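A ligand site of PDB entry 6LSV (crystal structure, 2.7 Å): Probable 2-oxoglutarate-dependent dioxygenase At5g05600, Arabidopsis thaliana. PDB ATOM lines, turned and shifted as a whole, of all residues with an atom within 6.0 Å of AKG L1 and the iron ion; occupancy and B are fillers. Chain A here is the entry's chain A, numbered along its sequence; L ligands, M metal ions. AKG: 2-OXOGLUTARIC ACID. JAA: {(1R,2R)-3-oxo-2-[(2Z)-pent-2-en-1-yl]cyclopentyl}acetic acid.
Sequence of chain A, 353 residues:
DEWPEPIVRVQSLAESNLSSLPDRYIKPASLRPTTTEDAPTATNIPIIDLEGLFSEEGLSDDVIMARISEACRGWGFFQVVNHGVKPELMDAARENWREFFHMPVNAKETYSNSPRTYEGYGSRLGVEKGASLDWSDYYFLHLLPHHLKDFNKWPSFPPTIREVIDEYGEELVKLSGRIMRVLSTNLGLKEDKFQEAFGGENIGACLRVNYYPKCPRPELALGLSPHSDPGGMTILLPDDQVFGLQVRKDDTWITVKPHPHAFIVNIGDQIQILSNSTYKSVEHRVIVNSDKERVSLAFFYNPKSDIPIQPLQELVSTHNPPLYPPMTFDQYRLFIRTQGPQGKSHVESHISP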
ATOM      1  N   ARG A 208     -16.935 -17.992   7.247  1.00  0.00           N
ATOM      2  CA  ARG A 208     -16.116 -16.811   7.033  1.00  0.00           C
ATOM      3  C   ARG A 208     -15.396 -16.492   8.321  1.00  0.00           C
ATOM      4  O   ARG A 208     -16.036 -16.299   9.360  1.00  0.00           O
ATOM      5  CB  ARG A 208     -16.940 -15.607   6.570  1.00  0.00           C
ATOM      6  CG  ARG A 208     -16.246 -14.284   6.862  1.00  0.00           C
ATOM      7  CD  ARG A 208     -16.706 -13.155   5.971  1.00  0.00           C
ATOM      8  NE  ARG A 208     -16.171 -11.881   6.442  1.00  0.00           N
ATOM      9  CZ  ARG A 208     -16.048 -10.787   5.695  1.00  0.00           C
ATOM     10  NH1 ARG A 208     -16.418 -10.815   4.425  1.00  0.00           N
ATOM     11  NH2 ARG A 208     -15.560  -9.669   6.213  1.00  0.00           N
ATOM     12  N   ASN A 210     -12.788 -13.883  10.231  1.00  0.00           N
ATOM     13  CA  ASN A 210     -12.464 -12.466  10.135  1.00  0.00           C
ATOM     14  C   ASN A 210     -11.224 -12.154  10.970  1.00  0.00           C
ATOM     15  O   ASN A 210     -11.132 -12.570  12.130  1.00  0.00           O
ATOM     16  CB  ASN A 210     -13.631 -11.605  10.589  1.00  0.00           C
ATOM     17  CG  ASN A 210     -14.886 -11.834   9.771  1.00  0.00           C
ATOM     18  OD1 ASN A 210     -14.848 -11.774   8.538  1.00  0.00           O
ATOM     19  ND2 ASN A 210     -15.995 -12.094  10.446  1.00  0.00           N
ATOM     20  N   TYR A 212      -8.980  -8.989  12.371  1.00  0.00           N
ATOM     21  CA  TYR A 212      -8.973  -7.546  12.633  1.00  0.00           C
ATOM     22  C   TYR A 212      -7.627  -7.163  13.220  1.00  0.00           C
ATOM     23  O   TYR A 212      -7.440  -7.210  14.451  1.00  0.00           O
ATOM     24  CB  TYR A 212     -10.110  -7.164  13.589  1.00  0.00           C
ATOM     25  CG  TYR A 212     -11.456  -7.724  13.181  1.00  0.00           C
ATOM     26  CD1 TYR A 212     -12.236  -7.082  12.234  1.00  0.00           C
ATOM     27  CD2 TYR A 212     -11.932  -8.909  13.728  1.00  0.00           C
ATOM     28  CE1 TYR A 212     -13.466  -7.588  11.845  1.00  0.00           C
ATOM     29  CE2 TYR A 212     -13.161  -9.427  13.347  1.00  0.00           C
ATOM     30  CZ  TYR A 212     -13.920  -8.764  12.412  1.00  0.00           C
ATOM     31  OH  TYR A 212     -15.138  -9.273  12.030  1.00  0.00           O
ATOM     32  N   LEU A 224     -15.606  -3.981  10.661  1.00  0.00           N
ATOM     33  CA  LEU A 224     -16.654  -4.430   9.749  1.00  0.00           C
ATOM     34  C   LEU A 224     -17.843  -3.485   9.907  1.00  0.00           C
ATOM     35  O   LEU A 224     -18.365  -3.312  11.009  1.00  0.00           O
ATOM     36  CB  LEU A 224     -17.055  -5.869  10.059  1.00  0.00           C
ATOM     37  CG  LEU A 224     -17.849  -6.627   9.002  1.00  0.00           C
ATOM     38  CD1 LEU A 224     -17.215  -6.471   7.627  1.00  0.00           C
ATOM     39  CD2 LEU A 224     -17.951  -8.096   9.397  1.00  0.00           C
ATOM     40  N   HIS A 227     -24.264  -4.257   9.255  1.00  0.00           N
ATOM     41  CA  HIS A 227     -24.961  -5.173   8.363  1.00  0.00           C
ATOM     42  C   HIS A 227     -25.723  -6.193   9.201  1.00  0.00           C
ATOM     43  O   HIS A 227     -25.388  -6.443  10.370  1.00  0.00           O
ATOM     44  CB  HIS A 227     -24.010  -5.910   7.424  1.00  0.00           C
ATOM     45  CG  HIS A 227     -23.194  -6.968   8.103  1.00  0.00           C
ATOM     46  ND1 HIS A 227     -22.246  -6.668   9.066  1.00  0.00           N
ATOM     47  CD2 HIS A 227     -23.198  -8.306   7.978  1.00  0.00           C
ATOM     48  CE1 HIS A 227     -21.698  -7.788   9.502  1.00  0.00           C
ATOM     49  NE2 HIS A 227     -22.255  -8.797   8.854  1.00  0.00           N
ATOM     50  N   SER A 228     -26.735  -6.794   8.588  1.00  0.00           N
ATOM     51  CA  SER A 228     -27.293  -8.054   9.049  1.00  0.00           C
ATOM     52  C   SER A 228     -26.840  -9.148   8.095  1.00  0.00           C
ATOM     53  O   SER A 228     -26.581  -8.894   6.909  1.00  0.00           O
ATOM     54  CB  SER A 228     -28.824  -8.000   9.128  1.00  0.00           C
ATOM     55  OG  SER A 228     -29.402  -7.642   7.888  1.00  0.00           O
ATOM     56  N   ASP A 229     -26.730 -10.365   8.615  1.00  0.00           N
ATOM     57  CA  ASP A 229     -26.271 -11.475   7.792  1.00  0.00           C
ATOM     58  C   ASP A 229     -27.348 -11.857   6.785  1.00  0.00           C
ATOM     59  O   ASP A 229     -28.518 -12.001   7.165  1.00  0.00           O
ATOM     60  CB  ASP A 229     -25.909 -12.666   8.673  1.00  0.00           C
ATOM     61  CG  ASP A 229     -24.707 -12.383   9.546  1.00  0.00           C
ATOM     62  OD1 ASP A 229     -23.808 -11.654   9.091  1.00  0.00           O
ATOM     63  OD2 ASP A 229     -24.668 -12.890  10.687  1.00  0.00           O
ATOM     64  N   THR A 234     -26.572 -17.290  11.769  1.00  0.00           N
ATOM     65  CA  THR A 234     -25.133 -17.293  11.944  1.00  0.00           C
ATOM     66  C   THR A 234     -24.789 -17.812  13.332  1.00  0.00           C
ATOM     67  O   THR A 234     -25.392 -17.376  14.320  1.00  0.00           O
ATOM     68  CB  THR A 234     -24.550 -15.888  11.751  1.00  0.00           C
ATOM     69  OG1 THR A 234     -24.980 -15.357  10.494  1.00  0.00           O
ATOM     70  CG2 THR A 234     -23.021 -15.940  11.778  1.00  0.00           C
ATOM     71  N   LEU A 236     -21.748 -17.558  15.644  1.00  0.00           N
ATOM     72  CA  LEU A 236     -20.571 -16.700  15.717  1.00  0.00           C
ATOM     73  C   LEU A 236     -19.721 -17.091  16.912  1.00  0.00           C
ATOM     74  O   LEU A 236     -20.224 -17.181  18.041  1.00  0.00           O
ATOM     75  CB  LEU A 236     -21.001 -15.227  15.832  1.00  0.00           C
ATOM     76  CG  LEU A 236     -19.960 -14.113  15.990  1.00  0.00           C
ATOM     77  CD1 LEU A 236     -18.969 -14.115  14.838  1.00  0.00           C
ATOM     78  CD2 LEU A 236     -20.672 -12.763  16.076  1.00  0.00           C
ATOM     79  N   LEU A 237     -18.436 -17.352  16.665  1.00  0.00           N
ATOM     80  CA  LEU A 237     -17.463 -17.571  17.730  1.00  0.00           C
ATOM     81  C   LEU A 237     -16.594 -16.325  17.815  1.00  0.00           C
ATOM     82  O   LEU A 237     -15.582 -16.214  17.100  1.00  0.00           O
ATOM     83  CB  LEU A 237     -16.616 -18.811  17.477  1.00  0.00           C
ATOM     84  CG  LEU A 237     -15.598 -19.133  18.577  1.00  0.00           C
ATOM     85  CD1 LEU A 237     -16.257 -19.068  19.952  1.00  0.00           C
ATOM     86  CD2 LEU A 237     -14.941 -20.486  18.354  1.00  0.00           C
ATOM     87  N   PRO A 238     -16.949 -15.352  18.644  1.00  0.00           N
ATOM     88  CA  PRO A 238     -16.153 -14.119  18.722  1.00  0.00           C
ATOM     89  C   PRO A 238     -14.854 -14.350  19.470  1.00  0.00           C
ATOM     90  O   PRO A 238     -14.694 -15.326  20.204  1.00  0.00           O
ATOM     91  CB  PRO A 238     -17.070 -13.150  19.470  1.00  0.00           C
ATOM     92  CG  PRO A 238     -17.946 -14.031  20.294  1.00  0.00           C
ATOM     93  CD  PRO A 238     -18.106 -15.333  19.560  1.00  0.00           C
ATOM     94  N   ASP A 239     -13.923 -13.433  19.257  1.00  0.00           N
ATOM     95  CA  ASP A 239     -12.595 -13.539  19.862  1.00  0.00           C
ATOM     96  C   ASP A 239     -12.721 -13.636  21.375  1.00  0.00           C
ATOM     97  O   ASP A 239     -13.316 -12.771  22.024  1.00  0.00           O
ATOM     98  CB  ASP A 239     -11.740 -12.339  19.468  1.00  0.00           C
ATOM     99  CG  ASP A 239     -10.270 -12.534  19.797  1.00  0.00           C
ATOM    100  OD1 ASP A 239      -9.916 -12.411  20.983  1.00  0.00           O
ATOM    101  OD2 ASP A 239      -9.487 -12.825  18.867  1.00  0.00           O
ATOM    102  N   GLY A 244     -14.954  -6.267  20.587  1.00  0.00           N
ATOM    103  CA  GLY A 244     -15.022  -5.590  19.309  1.00  0.00           C
ATOM    104  C   GLY A 244     -16.372  -5.734  18.627  1.00  0.00           C
ATOM    105  O   GLY A 244     -16.787  -4.856  17.870  1.00  0.00           O
ATOM    106  N   LEU A 245     -17.067  -6.836  18.893  1.00  0.00           N
ATOM    107  CA  LEU A 245     -18.374  -7.050  18.300  1.00  0.00           C
ATOM    108  C   LEU A 245     -19.406  -6.132  18.951  1.00  0.00           C
ATOM    109  O   LEU A 245     -19.478  -6.048  20.178  1.00  0.00           O
ATOM    110  CB  LEU A 245     -18.787  -8.513  18.442  1.00  0.00           C
ATOM    111  CG  LEU A 245     -20.246  -8.812  18.097  1.00  0.00           C
ATOM    112  CD1 LEU A 245     -20.455  -8.785  16.597  1.00  0.00           C
ATOM    113  CD2 LEU A 245     -20.640 -10.149  18.680  1.00  0.00           C
ATOM    114  N   ASN A 266     -27.019 -15.696  15.662  1.00  0.00           N
ATOM    115  CA  ASN A 266     -27.568 -14.532  14.992  1.00  0.00           C
ATOM    116  C   ASN A 266     -28.712 -14.958  14.089  1.00  0.00           C
ATOM    117  O   ASN A 266     -28.550 -15.863  13.259  1.00  0.00           O
ATOM    118  CB  ASN A 266     -26.506 -13.796  14.164  1.00  0.00           C
ATOM    119  CG  ASN A 266     -25.551 -12.992  15.014  1.00  0.00           C
ATOM    120  OD1 ASN A 266     -25.811 -12.734  16.192  1.00  0.00           O
ATOM    121  ND2 ASN A 266     -24.444 -12.573  14.419  1.00  0.00           N
ATOM    122  N   HIS A 284     -25.130  -5.849  13.234  1.00  0.00           N
ATOM    123  CA  HIS A 284     -23.899  -5.798  14.009  1.00  0.00           C
ATOM    124  C   HIS A 284     -22.787  -5.149  13.200  1.00  0.00           C
ATOM    125  O   HIS A 284     -22.881  -4.960  11.990  1.00  0.00           O
ATOM    126  CB  HIS A 284     -23.476  -7.201  14.476  1.00  0.00           C
ATOM    127  CG  HIS A 284     -23.711  -8.274  13.469  1.00  0.00           C
ATOM    128  ND1 HIS A 284     -24.958  -8.802  13.217  1.00  0.00           N
ATOM    129  CD2 HIS A 284     -22.856  -8.944  12.654  1.00  0.00           C
ATOM    130  CE1 HIS A 284     -24.868  -9.732  12.281  1.00  0.00           C
ATOM    131  NE2 HIS A 284     -23.600  -9.835  11.929  1.00  0.00           N
ATOM    132  N   ARG A 285     -21.725  -4.797  13.925  1.00  0.00           N
ATOM    133  CA  ARG A 285     -20.524  -4.193  13.360  1.00  0.00           C
ATOM    134  C   ARG A 285     -19.378  -4.533  14.302  1.00  0.00           C
ATOM    135  O   ARG A 285     -19.575  -4.912  15.455  1.00  0.00           O
ATOM    136  CB  ARG A 285     -20.674  -2.686  13.202  1.00  0.00           C
ATOM    137  CG  ARG A 285     -20.572  -1.917  14.506  1.00  0.00           C
ATOM    138  CD  ARG A 285     -20.710  -0.417  14.314  1.00  0.00           C
ATOM    139  NE  ARG A 285     -20.396   0.300  15.546  1.00  0.00           N
ATOM    140  CZ  ARG A 285     -20.530   1.615  15.705  1.00  0.00           C
ATOM    141  NH1 ARG A 285     -20.967   2.369  14.720  1.00  0.00           N
ATOM    142  NH2 ARG A 285     -20.215   2.174  16.872  1.00  0.00           N
ATOM    143  N   VAL A 286     -18.153  -4.399  13.797  1.00  0.00           N
ATOM    144  CA  VAL A 286     -16.952  -4.686  14.578  1.00  0.00           C
ATOM    145  C   VAL A 286     -16.134  -3.402  14.685  1.00  0.00           C
ATOM    146  O   VAL A 286     -15.911  -2.719  13.680  1.00  0.00           O
ATOM    147  CB  VAL A 286     -16.123  -5.822  13.962  1.00  0.00           C
ATOM    148  CG1 VAL A 286     -15.025  -6.255  14.929  1.00  0.00           C
ATOM    149  CG2 VAL A 286     -17.013  -7.006  13.611  1.00  0.00           C
ATOM    150  N   ARG A 294      -7.958  -9.221  16.668  1.00  0.00           N
ATOM    151  CA  ARG A 294      -9.108 -10.066  16.958  1.00  0.00           C
ATOM    152  C   ARG A 294      -9.203 -11.131  15.883  1.00  0.00           C
ATOM    153  O   ARG A 294      -8.771 -10.929  14.746  1.00  0.00           O
ATOM    154  CB  ARG A 294     -10.425  -9.263  17.029  1.00  0.00           C
ATOM    155  CG  ARG A 294     -10.647  -8.503  18.331  1.00  0.00           C
ATOM    156  CD  ARG A 294     -12.041  -7.878  18.415  1.00  0.00           C
ATOM    157  NE  ARG A 294     -13.071  -8.826  18.822  1.00  0.00           N
ATOM    158  CZ  ARG A 294     -13.984  -9.344  18.001  1.00  0.00           C
ATOM    159  NH1 ARG A 294     -14.001  -9.014  16.719  1.00  0.00           N
ATOM    160  NH2 ARG A 294     -14.879 -10.215  18.467  1.00  0.00           N
ATOM    161  N   VAL A 295      -9.774 -12.268  16.250  1.00  0.00           N
ATOM    162  CA  VAL A 295     -10.092 -13.337  15.304  1.00  0.00           C
ATOM    163  C   VAL A 295     -11.464 -13.884  15.664  1.00  0.00           C
ATOM    164  O   VAL A 295     -11.675 -14.334  16.797  1.00  0.00           O
ATOM    165  CB  VAL A 295      -9.052 -14.470  15.330  1.00  0.00           C
ATOM    166  CG1 VAL A 295      -9.632 -15.736  14.735  1.00  0.00           C
ATOM    167  CG2 VAL A 295      -7.786 -14.052  14.584  1.00  0.00           C
ATOM    168  N   SER A 296     -12.396 -13.827  14.721  1.00  0.00           N
ATOM    169  CA  SER A 296     -13.744 -14.318  14.939  1.00  0.00           C
ATOM    170  C   SER A 296     -14.157 -15.233  13.800  1.00  0.00           C
ATOM    171  O   SER A 296     -13.745 -15.052  12.649  1.00  0.00           O
ATOM    172  CB  SER A 296     -14.747 -13.167  15.083  1.00  0.00           C
ATOM    173  OG  SER A 296     -14.229 -12.160  15.944  1.00  0.00           O
ATOM    174  N   ALA A 298     -17.353 -16.928  11.763  1.00  0.00           N
ATOM    175  CA  ALA A 298     -18.761 -16.773  11.420  1.00  0.00           C
ATOM    176  C   ALA A 298     -19.193 -17.969  10.594  1.00  0.00           C
ATOM    177  O   ALA A 298     -18.802 -18.108   9.426  1.00  0.00           O
ATOM    178  CB  ALA A 298     -19.000 -15.465  10.664  1.00  0.00           C
ATOM    179  N   PHE A 300     -22.258 -19.773   8.746  1.00  0.00           N
ATOM    180  CA  PHE A 300     -23.529 -19.400   8.145  1.00  0.00           C
ATOM    181  C   PHE A 300     -24.329 -20.661   7.821  1.00  0.00           C
ATOM    182  O   PHE A 300     -23.849 -21.532   7.097  1.00  0.00           O
ATOM    183  CB  PHE A 300     -23.320 -18.565   6.885  1.00  0.00           C
ATOM    184  CG  PHE A 300     -22.479 -17.341   7.087  1.00  0.00           C
ATOM    185  CD1 PHE A 300     -22.898 -16.325   7.944  1.00  0.00           C
ATOM    186  CD2 PHE A 300     -21.275 -17.197   6.423  1.00  0.00           C
ATOM    187  CE1 PHE A 300     -22.116 -15.185   8.126  1.00  0.00           C
ATOM    188  CE2 PHE A 300     -20.504 -16.066   6.606  1.00  0.00           C
ATOM    189  CZ  PHE A 300     -20.921 -15.063   7.458  1.00  0.00           C
HETATM  190  C1  AKG L   1     -19.438 -11.509  10.917  1.00  0.00           C
HETATM  191  O1  AKG L   1     -20.537 -12.108  10.914  1.00  0.00           O
HETATM  192  O2  AKG L   1     -18.663 -11.627   9.923  1.00  0.00           O
HETATM  193  C2  AKG L   1     -19.056 -10.628  12.110  1.00  0.00           C
HETATM  194  O5  AKG L   1     -19.735  -9.683  12.362  1.00  0.00           O
HETATM  195  C3  AKG L   1     -17.829 -10.916  12.991  1.00  0.00           C
HETATM  196  C4  AKG L   1     -18.167 -10.576  14.449  1.00  0.00           C
HETATM  197  C5  AKG L   1     -16.892 -10.422  15.284  1.00  0.00           C
HETATM  198  O3  AKG L   1     -16.889 -10.677  16.514  1.00  0.00           O
HETATM  199  O4  AKG L   1     -15.834 -10.040  14.728  1.00  0.00           O
HETATM  200  O01 JAA L   2     -17.998 -12.828   2.908  1.00  0.00           O
HETATM  201  O02 JAA L   2     -23.253 -16.091   1.437  1.00  0.00           O
HETATM  202  O03 JAA L   2     -23.161 -14.874  -0.360  1.00  0.00           O
HETATM  203  C04 JAA L   2     -20.970 -14.118   1.919  1.00  0.00           C
HETATM  204  C05 JAA L   2     -20.215 -12.875   2.657  1.00  0.00           C
HETATM  205  C06 JAA L   2     -20.210 -14.250   0.570  1.00  0.00           C
HETATM  206  C07 JAA L   2     -19.026 -13.553   0.713  1.00  0.00           C
HETATM  207  C08 JAA L   2     -18.981 -13.028   2.267  1.00  0.00           C
HETATM  208  C09 JAA L   2     -20.330 -12.978   4.242  1.00  0.00           C
HETATM  209  C10 JAA L   2     -22.351 -13.854   1.692  1.00  0.00           C
HETATM  210  C11 JAA L   2     -21.610 -12.297   4.722  1.00  0.00           C
HETATM  211  C12 JAA L   2     -22.958 -15.002   0.882  1.00  0.00           C
HETATM  212  C13 JAA L   2     -21.607 -11.423   5.711  1.00  0.00           C
HETATM  213  C14 JAA L   2     -20.315 -11.052   6.440  1.00  0.00           C
HETATM  214  C15 JAA L   2     -20.155  -9.536   6.462  1.00  0.00           C
HETATM  215 FE    FE M   1     -21.837 -10.732  10.215  1.00  0.00          FE
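The side-chain amide nitrogen (ND2) of Asn 210 lies within hydrogen-bond range of an oxygen (O2) of AKG L1, 2.8 Å away.
An oxygen (O3) of AKG L1 is in salt-bridge range of the guanidinium group of Arg 294 (2.8 Å).
OH of Tyr 212 sits at hydrogen-bond distance from O4 of AKG L1, at 2.9 Å.
The side-chain hydroxyl (OG) of Ser 296 lies within hydrogen-bond range of an oxygen (O4) of AKG L1, at 2.9 Å.
NH1 of Arg 208 lies within hydrogen-bond range of O01 of JAA L2, 3.0 Å away.
The side-chain hydroxyl (OG1) of Thr 234 is in hydrogen-bond range of the side-chain carboxylate (OD2) of Asp 229, 2.5 Å away.
The side-chain amide nitrogen of Asn 210 lies close to the side-chain hydroxyl of Tyr 212 (3.3 Å).
The backbone NH (N) of Asn 210 is in hydrogen-bond range of the backbone carbonyl oxygen (O) of Ser 296 (2.9 Å).
OD1 of Asn 210 sits at hydrogen-bond distance from NE of Arg 208, 2.5 Å away.
The backbone NH (N) of Arg 294 is in hydrogen-bond range of the backbone carbonyl oxygen (O) of Tyr 212 (3.0 Å).
The side-chain hydroxyl (OG) of Ser 296 sits at hydrogen-bond distance from the guanidinium group (NH1) of Arg 294, at 3.2 Å.
The backbone carbonyl oxygen (O) of Leu 224 is in hydrogen-bond range of the backbone NH (N) of Val 286 (3.0 Å).
The backbone NH (N) of Ala 298 is in hydrogen-bond range of the backbone carbonyl oxygen (O) of Arg 208, at 2.8 Å.
Leu 224 touches AKG L1 (CD2 to O2, 3.6 Å).
Leu 236 touches AKG L1.
Pro 238 touches AKG L1 (CB to O3, 3.9 Å).
Leu 245 touches AKG L1.
CG2 of Val 286 touches O4 of AKG L1, at 3.4 Å.
Ala 298 touches AKG L1.
The nearest printed residue that does not touch AKG L1 is Arg 208 (4.3 Å).
The nearest printed residue that does not touch the iron ion is Leu 224 (4.8 Å).
An oxygen (O1) of AKG L1 is bound to the iron ion (2.0 Å).
The iron ion is bound by a ring nitrogen (NE2) of His 227, at 2.4 Å.
The side-chain carboxylate (OD1) of Asp 229 binds the iron ion (2.4 Å).
A ring nitrogen (NE2) of His 284 binds the iron ion.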
